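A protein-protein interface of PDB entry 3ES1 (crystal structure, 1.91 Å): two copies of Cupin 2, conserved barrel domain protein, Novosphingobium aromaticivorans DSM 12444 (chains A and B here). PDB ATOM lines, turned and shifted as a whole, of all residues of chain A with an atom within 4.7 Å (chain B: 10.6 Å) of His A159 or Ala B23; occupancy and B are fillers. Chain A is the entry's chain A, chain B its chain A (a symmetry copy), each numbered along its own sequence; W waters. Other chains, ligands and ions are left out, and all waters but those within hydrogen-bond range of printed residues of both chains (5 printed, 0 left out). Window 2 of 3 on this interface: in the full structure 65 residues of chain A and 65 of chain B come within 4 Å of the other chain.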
ATOM      1  N   TYR A 157      19.958  -0.597  21.898  1.00  0.00           N
ATOM      2  CA  TYR A 157      20.315  -1.516  20.857  1.00  0.00           C
ATOM      3  C   TYR A 157      19.056  -2.292  20.504  1.00  0.00           C
ATOM      4  O   TYR A 157      18.314  -2.768  21.385  1.00  0.00           O
ATOM      5  CB  TYR A 157      21.455  -2.472  21.278  1.00  0.00           C
ATOM      6  CG  TYR A 157      21.721  -3.497  20.202  1.00  0.00           C
ATOM      7  CD1 TYR A 157      22.455  -3.149  19.069  1.00  0.00           C
ATOM      8  CD2 TYR A 157      21.167  -4.776  20.262  1.00  0.00           C
ATOM      9  CE1 TYR A 157      22.684  -4.064  18.059  1.00  0.00           C
ATOM     10  CE2 TYR A 157      21.372  -5.697  19.231  1.00  0.00           C
ATOM     11  CZ  TYR A 157      22.150  -5.330  18.150  1.00  0.00           C
ATOM     12  OH  TYR A 157      22.329  -6.207  17.098  1.00  0.00           O
ATOM     13  N   LEU A 158      18.850  -2.408  19.202  1.00  0.00           N
ATOM     14  CA  LEU A 158      17.716  -3.153  18.623  1.00  0.00           C
ATOM     15  C   LEU A 158      18.132  -4.531  18.078  1.00  0.00           C
ATOM     16  O   LEU A 158      18.904  -4.671  17.119  1.00  0.00           O
ATOM     17  CB  LEU A 158      17.007  -2.331  17.535  1.00  0.00           C
ATOM     18  CG  LEU A 158      16.279  -1.049  17.967  1.00  0.00           C
ATOM     19  CD1 LEU A 158      15.610  -0.318  16.777  1.00  0.00           C
ATOM     20  CD2 LEU A 158      15.291  -1.347  19.055  1.00  0.00           C
ATOM     21  N   HIS A 159      17.589  -5.552  18.717  1.00  0.00           N
ATOM     22  CA  HIS A 159      17.691  -6.934  18.248  1.00  0.00           C
ATOM     23  C   HIS A 159      16.357  -7.416  17.676  1.00  0.00           C
ATOM     24  O   HIS A 159      15.358  -7.467  18.379  1.00  0.00           O
ATOM     25  CB  HIS A 159      18.095  -7.836  19.396  1.00  0.00           C
ATOM     26  CG  HIS A 159      18.204  -9.274  19.020  1.00  0.00           C
ATOM     27  ND1 HIS A 159      19.119  -9.723  18.103  1.00  0.00           N
ATOM     28  CD2 HIS A 159      17.522 -10.364  19.439  1.00  0.00           C
ATOM     29  CE1 HIS A 159      18.993 -11.029  17.962  1.00  0.00           C
ATOM     30  NE2 HIS A 159      18.023 -11.440  18.749  1.00  0.00           N
ATOM     31  N   ASN A 160      16.397  -7.775  16.403  1.00  0.00           N
ATOM     32  CA  ASN A 160      15.210  -8.101  15.612  1.00  0.00           C
ATOM     33  C   ASN A 160      14.184  -7.007  15.842  1.00  0.00           C
ATOM     34  O   ASN A 160      13.027  -7.277  16.180  1.00  0.00           O
ATOM     35  CB  ASN A 160      14.625  -9.445  16.037  1.00  0.00           C
ATOM     36  CG  ASN A 160      15.533 -10.629  15.700  1.00  0.00           C
ATOM     37  OD1 ASN A 160      16.282 -10.624  14.703  1.00  0.00           O
ATOM     38  ND2 ASN A 160      15.465 -11.658  16.557  1.00  0.00           N
ATOM     39  N   GLY A 161      14.678  -5.773  15.807  1.00  0.00           N
ATOM     40  CA  GLY A 161      13.833  -4.576  15.893  1.00  0.00           C
ATOM     41  C   GLY A 161      13.262  -4.282  17.257  1.00  0.00           C
ATOM     42  O   GLY A 161      12.420  -3.411  17.407  1.00  0.00           O
ATOM     43  N   GLN A 162      13.732  -5.006  18.260  1.00  0.00           N
ATOM     44  CA  GLN A 162      13.270  -4.789  19.627  1.00  0.00           C
ATOM     45  C   GLN A 162      14.430  -4.673  20.589  1.00  0.00           C
ATOM     46  O   GLN A 162      15.491  -5.231  20.340  1.00  0.00           O
ATOM     47  CB  GLN A 162      12.414  -5.955  20.117  1.00  0.00           C
ATOM     48  CG  GLN A 162      11.158  -6.242  19.323  1.00  0.00           C
ATOM     49  CD  GLN A 162      10.221  -5.064  19.258  1.00  0.00           C
ATOM     50  OE1 GLN A 162       9.906  -4.431  20.270  1.00  0.00           O
ATOM     51  NE2 GLN A 162       9.757  -4.762  18.053  1.00  0.00           N
ATOM     52  N   LEU A 164      16.736  -5.427  23.853  1.00  0.00           N
ATOM     53  CA  LEU A 164      17.102  -6.669  24.536  1.00  0.00           C
ATOM     54  C   LEU A 164      16.509  -6.756  25.974  1.00  0.00           C
ATOM     55  O   LEU A 164      16.342  -5.756  26.668  1.00  0.00           O
ATOM     56  CB  LEU A 164      18.615  -6.802  24.665  1.00  0.00           C
ATOM     57  CG  LEU A 164      19.517  -6.749  23.449  1.00  0.00           C
ATOM     58  CD1 LEU A 164      20.938  -6.427  23.901  1.00  0.00           C
ATOM     59  CD2 LEU A 164      19.438  -8.084  22.732  1.00  0.00           C
ATOM     60  N   GLY B  20      30.376  -5.780  19.907  1.00  0.00           N
ATOM     61  CA  GLY B  20      29.137  -5.751  19.121  1.00  0.00           C
ATOM     62  C   GLY B  20      28.194  -6.846  19.570  1.00  0.00           C
ATOM     63  O   GLY B  20      28.466  -7.541  20.544  1.00  0.00           O
ATOM     64  N   HIS B  21      27.108  -7.001  18.820  1.00  0.00           N
ATOM     65  CA  HIS B  21      26.092  -8.038  19.082  1.00  0.00           C
ATOM     66  C   HIS B  21      26.024  -8.996  17.926  1.00  0.00           C
ATOM     67  O   HIS B  21      26.211  -8.597  16.767  1.00  0.00           O
ATOM     68  CB  HIS B  21      24.716  -7.390  19.266  1.00  0.00           C
ATOM     69  CG  HIS B  21      24.579  -6.614  20.527  1.00  0.00           C
ATOM     70  ND1 HIS B  21      24.841  -5.266  20.595  1.00  0.00           N
ATOM     71  CD2 HIS B  21      24.258  -7.004  21.786  1.00  0.00           C
ATOM     72  CE1 HIS B  21      24.687  -4.858  21.846  1.00  0.00           C
ATOM     73  NE2 HIS B  21      24.327  -5.889  22.587  1.00  0.00           N
ATOM     74  N   ASP B  22      25.808 -10.262  18.250  1.00  0.00           N
ATOM     75  CA  ASP B  22      25.669 -11.294  17.228  1.00  0.00           C
ATOM     76  C   ASP B  22      24.211 -11.490  16.847  1.00  0.00           C
ATOM     77  O   ASP B  22      23.323 -10.729  17.274  1.00  0.00           O
ATOM     78  CB  ASP B  22      26.401 -12.603  17.602  1.00  0.00           C
ATOM     79  CG  ASP B  22      25.724 -13.368  18.736  1.00  0.00           C
ATOM     80  OD1 ASP B  22      24.607 -12.961  19.076  1.00  0.00           O
ATOM     81  OD2 ASP B  22      26.304 -14.369  19.233  1.00  0.00           O
ATOM     82  N   ALA B  23      23.964 -12.492  16.015  1.00  0.00           N
ATOM     83  CA  ALA B  23      22.619 -12.684  15.453  1.00  0.00           C
ATOM     84  C   ALA B  23      21.674 -13.159  16.512  1.00  0.00           C
ATOM     85  O   ALA B  23      20.478 -13.201  16.302  1.00  0.00           O
ATOM     86  CB  ALA B  23      22.641 -13.693  14.294  1.00  0.00           C
ATOM     87  N   HIS B  24      22.232 -13.516  17.662  1.00  0.00           N
ATOM     88  CA  HIS B  24      21.463 -14.059  18.787  1.00  0.00           C
ATOM     89  C   HIS B  24      21.286 -13.020  19.839  1.00  0.00           C
ATOM     90  O   HIS B  24      20.724 -13.296  20.878  1.00  0.00           O
ATOM     91  CB  HIS B  24      22.150 -15.277  19.386  1.00  0.00           C
ATOM     92  CG  HIS B  24      22.315 -16.368  18.401  1.00  0.00           C
ATOM     93  ND1 HIS B  24      21.282 -17.218  18.068  1.00  0.00           N
ATOM     94  CD2 HIS B  24      23.356 -16.692  17.598  1.00  0.00           C
ATOM     95  CE1 HIS B  24      21.696 -18.045  17.124  1.00  0.00           C
ATOM     96  NE2 HIS B  24      22.948 -17.745  16.821  1.00  0.00           N
ATOM     97  N   GLY B  25      21.737 -11.807  19.536  1.00  0.00           N
ATOM     98  CA  GLY B  25      21.564 -10.669  20.444  1.00  0.00           C
ATOM     99  C   GLY B  25      22.520 -10.719  21.627  1.00  0.00           C
ATOM    100  O   GLY B  25      22.312 -10.071  22.654  1.00  0.00           O
ATOM    101  N   ARG B  26      23.553 -11.531  21.479  1.00  0.00           N
ATOM    102  CA  ARG B  26      24.641 -11.638  22.474  1.00  0.00           C
ATOM    103  C   ARG B  26      25.796 -10.661  22.238  1.00  0.00           C
ATOM    104  O   ARG B  26      26.187 -10.361  21.090  1.00  0.00           O
ATOM    105  CB  ARG B  26      25.175 -13.082  22.545  1.00  0.00           C
ATOM    106  CG  ARG B  26      24.075 -14.150  22.772  1.00  0.00           C
ATOM    107  CD  ARG B  26      23.098 -13.764  23.848  1.00  0.00           C
ATOM    108  NE  ARG B  26      23.636 -14.125  25.135  1.00  0.00           N
ATOM    109  CZ  ARG B  26      23.168 -13.707  26.300  1.00  0.00           C
ATOM    110  NH1 ARG B  26      22.110 -12.921  26.364  1.00  0.00           N
ATOM    111  NH2 ARG B  26      23.769 -14.089  27.416  1.00  0.00           N
ATOM    112  N   ALA B  27      26.342 -10.179  23.349  1.00  0.00           N
ATOM    113  CA  ALA B  27      27.532  -9.300  23.334  1.00  0.00           C
ATOM    114  C   ALA B  27      28.788 -10.142  23.121  1.00  0.00           C
ATOM    115  O   ALA B  27      29.095 -11.078  23.862  1.00  0.00           O
ATOM    116  CB  ALA B  27      27.626  -8.437  24.599  1.00  0.00           C
ATOM    117  N   VAL B  28      29.450  -9.810  22.025  1.00  0.00           N
ATOM    118  CA  VAL B  28      30.624 -10.502  21.539  1.00  0.00           C
ATOM    119  C   VAL B  28      31.701  -9.515  21.126  1.00  0.00           C
ATOM    120  O   VAL B  28      31.448  -8.311  21.036  1.00  0.00           O
ATOM    121  CB  VAL B  28      30.276 -11.371  20.293  1.00  0.00           C
ATOM    122  CG1 VAL B  28      29.135 -12.292  20.588  1.00  0.00           C
ATOM    123  CG2 VAL B  28      29.914 -10.507  19.082  1.00  0.00           C
ATOM    124  N   PHE B  29      32.899 -10.043  20.895  1.00  0.00           N
ATOM    125  CA  PHE B  29      34.020  -9.249  20.300  1.00  0.00           C
ATOM    126  C   PHE B  29      33.870  -9.203  18.793  1.00  0.00           C
ATOM    127  O   PHE B  29      33.709 -10.241  18.152  1.00  0.00           O
ATOM    128  CB  PHE B  29      35.399  -9.815  20.749  1.00  0.00           C
ATOM    129  CG  PHE B  29      35.634  -9.657  22.215  1.00  0.00           C
ATOM    130  CD1 PHE B  29      36.026  -8.442  22.739  1.00  0.00           C
ATOM    131  CD2 PHE B  29      35.428 -10.711  23.098  1.00  0.00           C
ATOM    132  CE1 PHE B  29      36.233  -8.310  24.128  1.00  0.00           C
ATOM    133  CE2 PHE B  29      35.588 -10.553  24.482  1.00  0.00           C
ATOM    134  CZ  PHE B  29      35.966  -9.354  24.983  1.00  0.00           C
ATOM    135  N   ASP B  59      24.874   5.333  17.090  1.00  0.00           N
ATOM    136  CA  ASP B  59      23.986   4.237  16.625  1.00  0.00           C
ATOM    137  C   ASP B  59      24.647   2.911  16.790  1.00  0.00           C
ATOM    138  O   ASP B  59      25.543   2.549  16.030  1.00  0.00           O
ATOM    139  CB  ASP B  59      23.642   4.421  15.144  1.00  0.00           C
ATOM    140  CG  ASP B  59      22.587   3.443  14.648  1.00  0.00           C
ATOM    141  OD1 ASP B  59      22.187   2.537  15.383  1.00  0.00           O
ATOM    142  OD2 ASP B  59      22.212   3.556  13.472  1.00  0.00           O
ATOM    143  N   ASN B  60      24.232   2.168  17.817  1.00  0.00           N
ATOM    144  CA  ASN B  60      24.849   0.869  18.013  1.00  0.00           C
ATOM    145  C   ASN B  60      24.231  -0.202  17.133  1.00  0.00           C
ATOM    146  O   ASN B  60      24.545  -1.394  17.273  1.00  0.00           O
ATOM    147  CB  ASN B  60      24.881   0.457  19.487  1.00  0.00           C
ATOM    148  CG  ASN B  60      25.883   1.249  20.243  1.00  0.00           C
ATOM    149  OD1 ASN B  60      27.002   1.488  19.754  1.00  0.00           O
ATOM    150  ND2 ASN B  60      25.515   1.698  21.407  1.00  0.00           N
ATOM    151  N   ASN B  61      23.369   0.219  16.217  1.00  0.00           N
ATOM    152  CA  ASN B  61      22.923  -0.686  15.110  1.00  0.00           C
ATOM    153  C   ASN B  61      23.645  -0.450  13.789  1.00  0.00           C
ATOM    154  O   ASN B  61      23.457  -1.172  12.787  1.00  0.00           O
ATOM    155  CB  ASN B  61      21.389  -0.658  14.927  1.00  0.00           C
ATOM    156  CG  ASN B  61      20.698  -1.633  15.864  1.00  0.00           C
ATOM    157  OD1 ASN B  61      20.501  -2.804  15.530  1.00  0.00           O
ATOM    158  ND2 ASN B  61      20.416  -1.181  17.066  1.00  0.00           N
ATOM    159  N   ASP B  62      24.566   0.500  13.832  1.00  0.00           N
ATOM    160  CA  ASP B  62      25.458   0.811  12.711  1.00  0.00           C
ATOM    161  C   ASP B  62      26.730  -0.004  12.862  1.00  0.00           C
ATOM    162  O   ASP B  62      27.544   0.247  13.741  1.00  0.00           O
ATOM    163  CB  ASP B  62      25.794   2.312  12.669  1.00  0.00           C
ATOM    164  CG  ASP B  62      26.730   2.681  11.531  1.00  0.00           C
ATOM    165  OD1 ASP B  62      27.022   1.803  10.691  1.00  0.00           O
ATOM    166  OD2 ASP B  62      27.201   3.844  11.496  1.00  0.00           O
ATOM    167  N   GLU B  63      26.847  -0.984  11.976  1.00  0.00           N
ATOM    168  CA  GLU B  63      27.899  -2.004  12.008  1.00  0.00           C
ATOM    169  C   GLU B  63      29.139  -1.556  11.238  1.00  0.00           C
ATOM    170  O   GLU B  63      30.133  -2.276  11.172  1.00  0.00           O
ATOM    171  CB  GLU B  63      27.338  -3.342  11.483  1.00  0.00           C
ATOM    172  CG  GLU B  63      26.212  -3.942  12.359  1.00  0.00           C
ATOM    173  CD  GLU B  63      26.623  -4.144  13.848  1.00  0.00           C
ATOM    174  OE1 GLU B  63      27.782  -4.627  14.051  1.00  0.00           O
ATOM    175  OE2 GLU B  63      25.809  -3.836  14.812  1.00  0.00           O
HETATM  176  O   HOH W   1      19.366 -11.551  14.494  1.00  0.00           O
HETATM  177  O   HOH W   2      21.319  -8.622  17.253  1.00  0.00           O
HETATM  178  O   HOH W   3      23.535  -5.051  14.678  1.00  0.00           O
HETATM  179  O   HOH W   4      22.832   1.247  22.626  1.00  0.00           O
HETATM  180  O   HOH W   5      17.212 -13.922  16.632  1.00  0.00           O
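The side-chain amide nitrogen (ND2) of Asn A160 lies within hydrogen-bond range of a ring nitrogen (NE2) of His A159 (3.4 Å). OD1 of Asp B22 is in hydrogen-bond range of N of His B24 (2.8 Å). OD1 of Asp B22 is in hydrogen-bond range of N of Gly B25 (3.1 Å). N of Asn B61 lies within hydrogen-bond range of OD1 of Asp B59, 2.7 Å away.
The backbone NH (N) of Leu A158 lies close to the side-chain amide nitrogen (ND2) of Asn B61 (2.9 Å).
No position is printed for both chains. Of the 9 pairs that touch across the chains among the printed residues, none has its exchanged pair printed and touching as well.
Water W3 bridges OE2 of Glu B63 (2.6 Å) and OH of Tyr A157 (2.9 Å). Water W2 lies within hydrogen-bond range of ND1 of His A159, OH of Tyr A157 and O of Asp B22. Water W1 bridges O of Ala B23 (2.7 Å) and OD1 of Asn A160 (3.2 Å). Water W5 lies within hydrogen-bond range of ND2 of Asn A160, O of Ala B23 and NE2 of His A159. Water W4 bridges ND2 of Asn B60 and N of Tyr A157.
Hydrophobic or aromatic side chains of chain B within 4 Å of the printed part of chain A: His B21. Of the 7 printed residues of chain A, 4 touch a printed residue of chain B. Hydrophobic or aromatic side chains of chain A that line the printed part of chain B: Tyr A157, Leu A158, His A159 and Leu A164. Along chain A the printed residues that touch a printed residue of chain B span positions 157 to 164. Among the printed residues, no Asp or Glu carboxylate lies within 4 Å of a Lys or Arg side-chain nitrogen of the other chain.
Leu A158 touches just one residue of chain B: Asn B61 (2.9 Å). Of chain B, only Ala B23, His B24 and Gly B25 come within 4 Å of His A159. No residue of chain B comes within 4 Å of Asn A160. No residue of chain B comes within 4 Å of Gly A161. Printed residues of chain A within 4 Å of His B21: Tyr A157 (3.4 Å) and Leu A164 (3.7 Å). Ala B23 touches just one residue of chain A: His A159 (3.1 Å). Val B28 touches none of the printed residues of chain A. Printed residues of chain A within 4 Å of Asn B61: Tyr A157 (3.5 Å) and Leu A158 (2.9 Å).
Among the printed residues, pairs that only touch across the chains: His A159 with Ala B23, His A159 with Gly B25, Tyr A157 with Asn B60, Tyr A157 with His B21, Tyr A157 with Asn B61, Leu A164 with Gly B25, His A159 with His B24 and Leu A164 with His B21.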
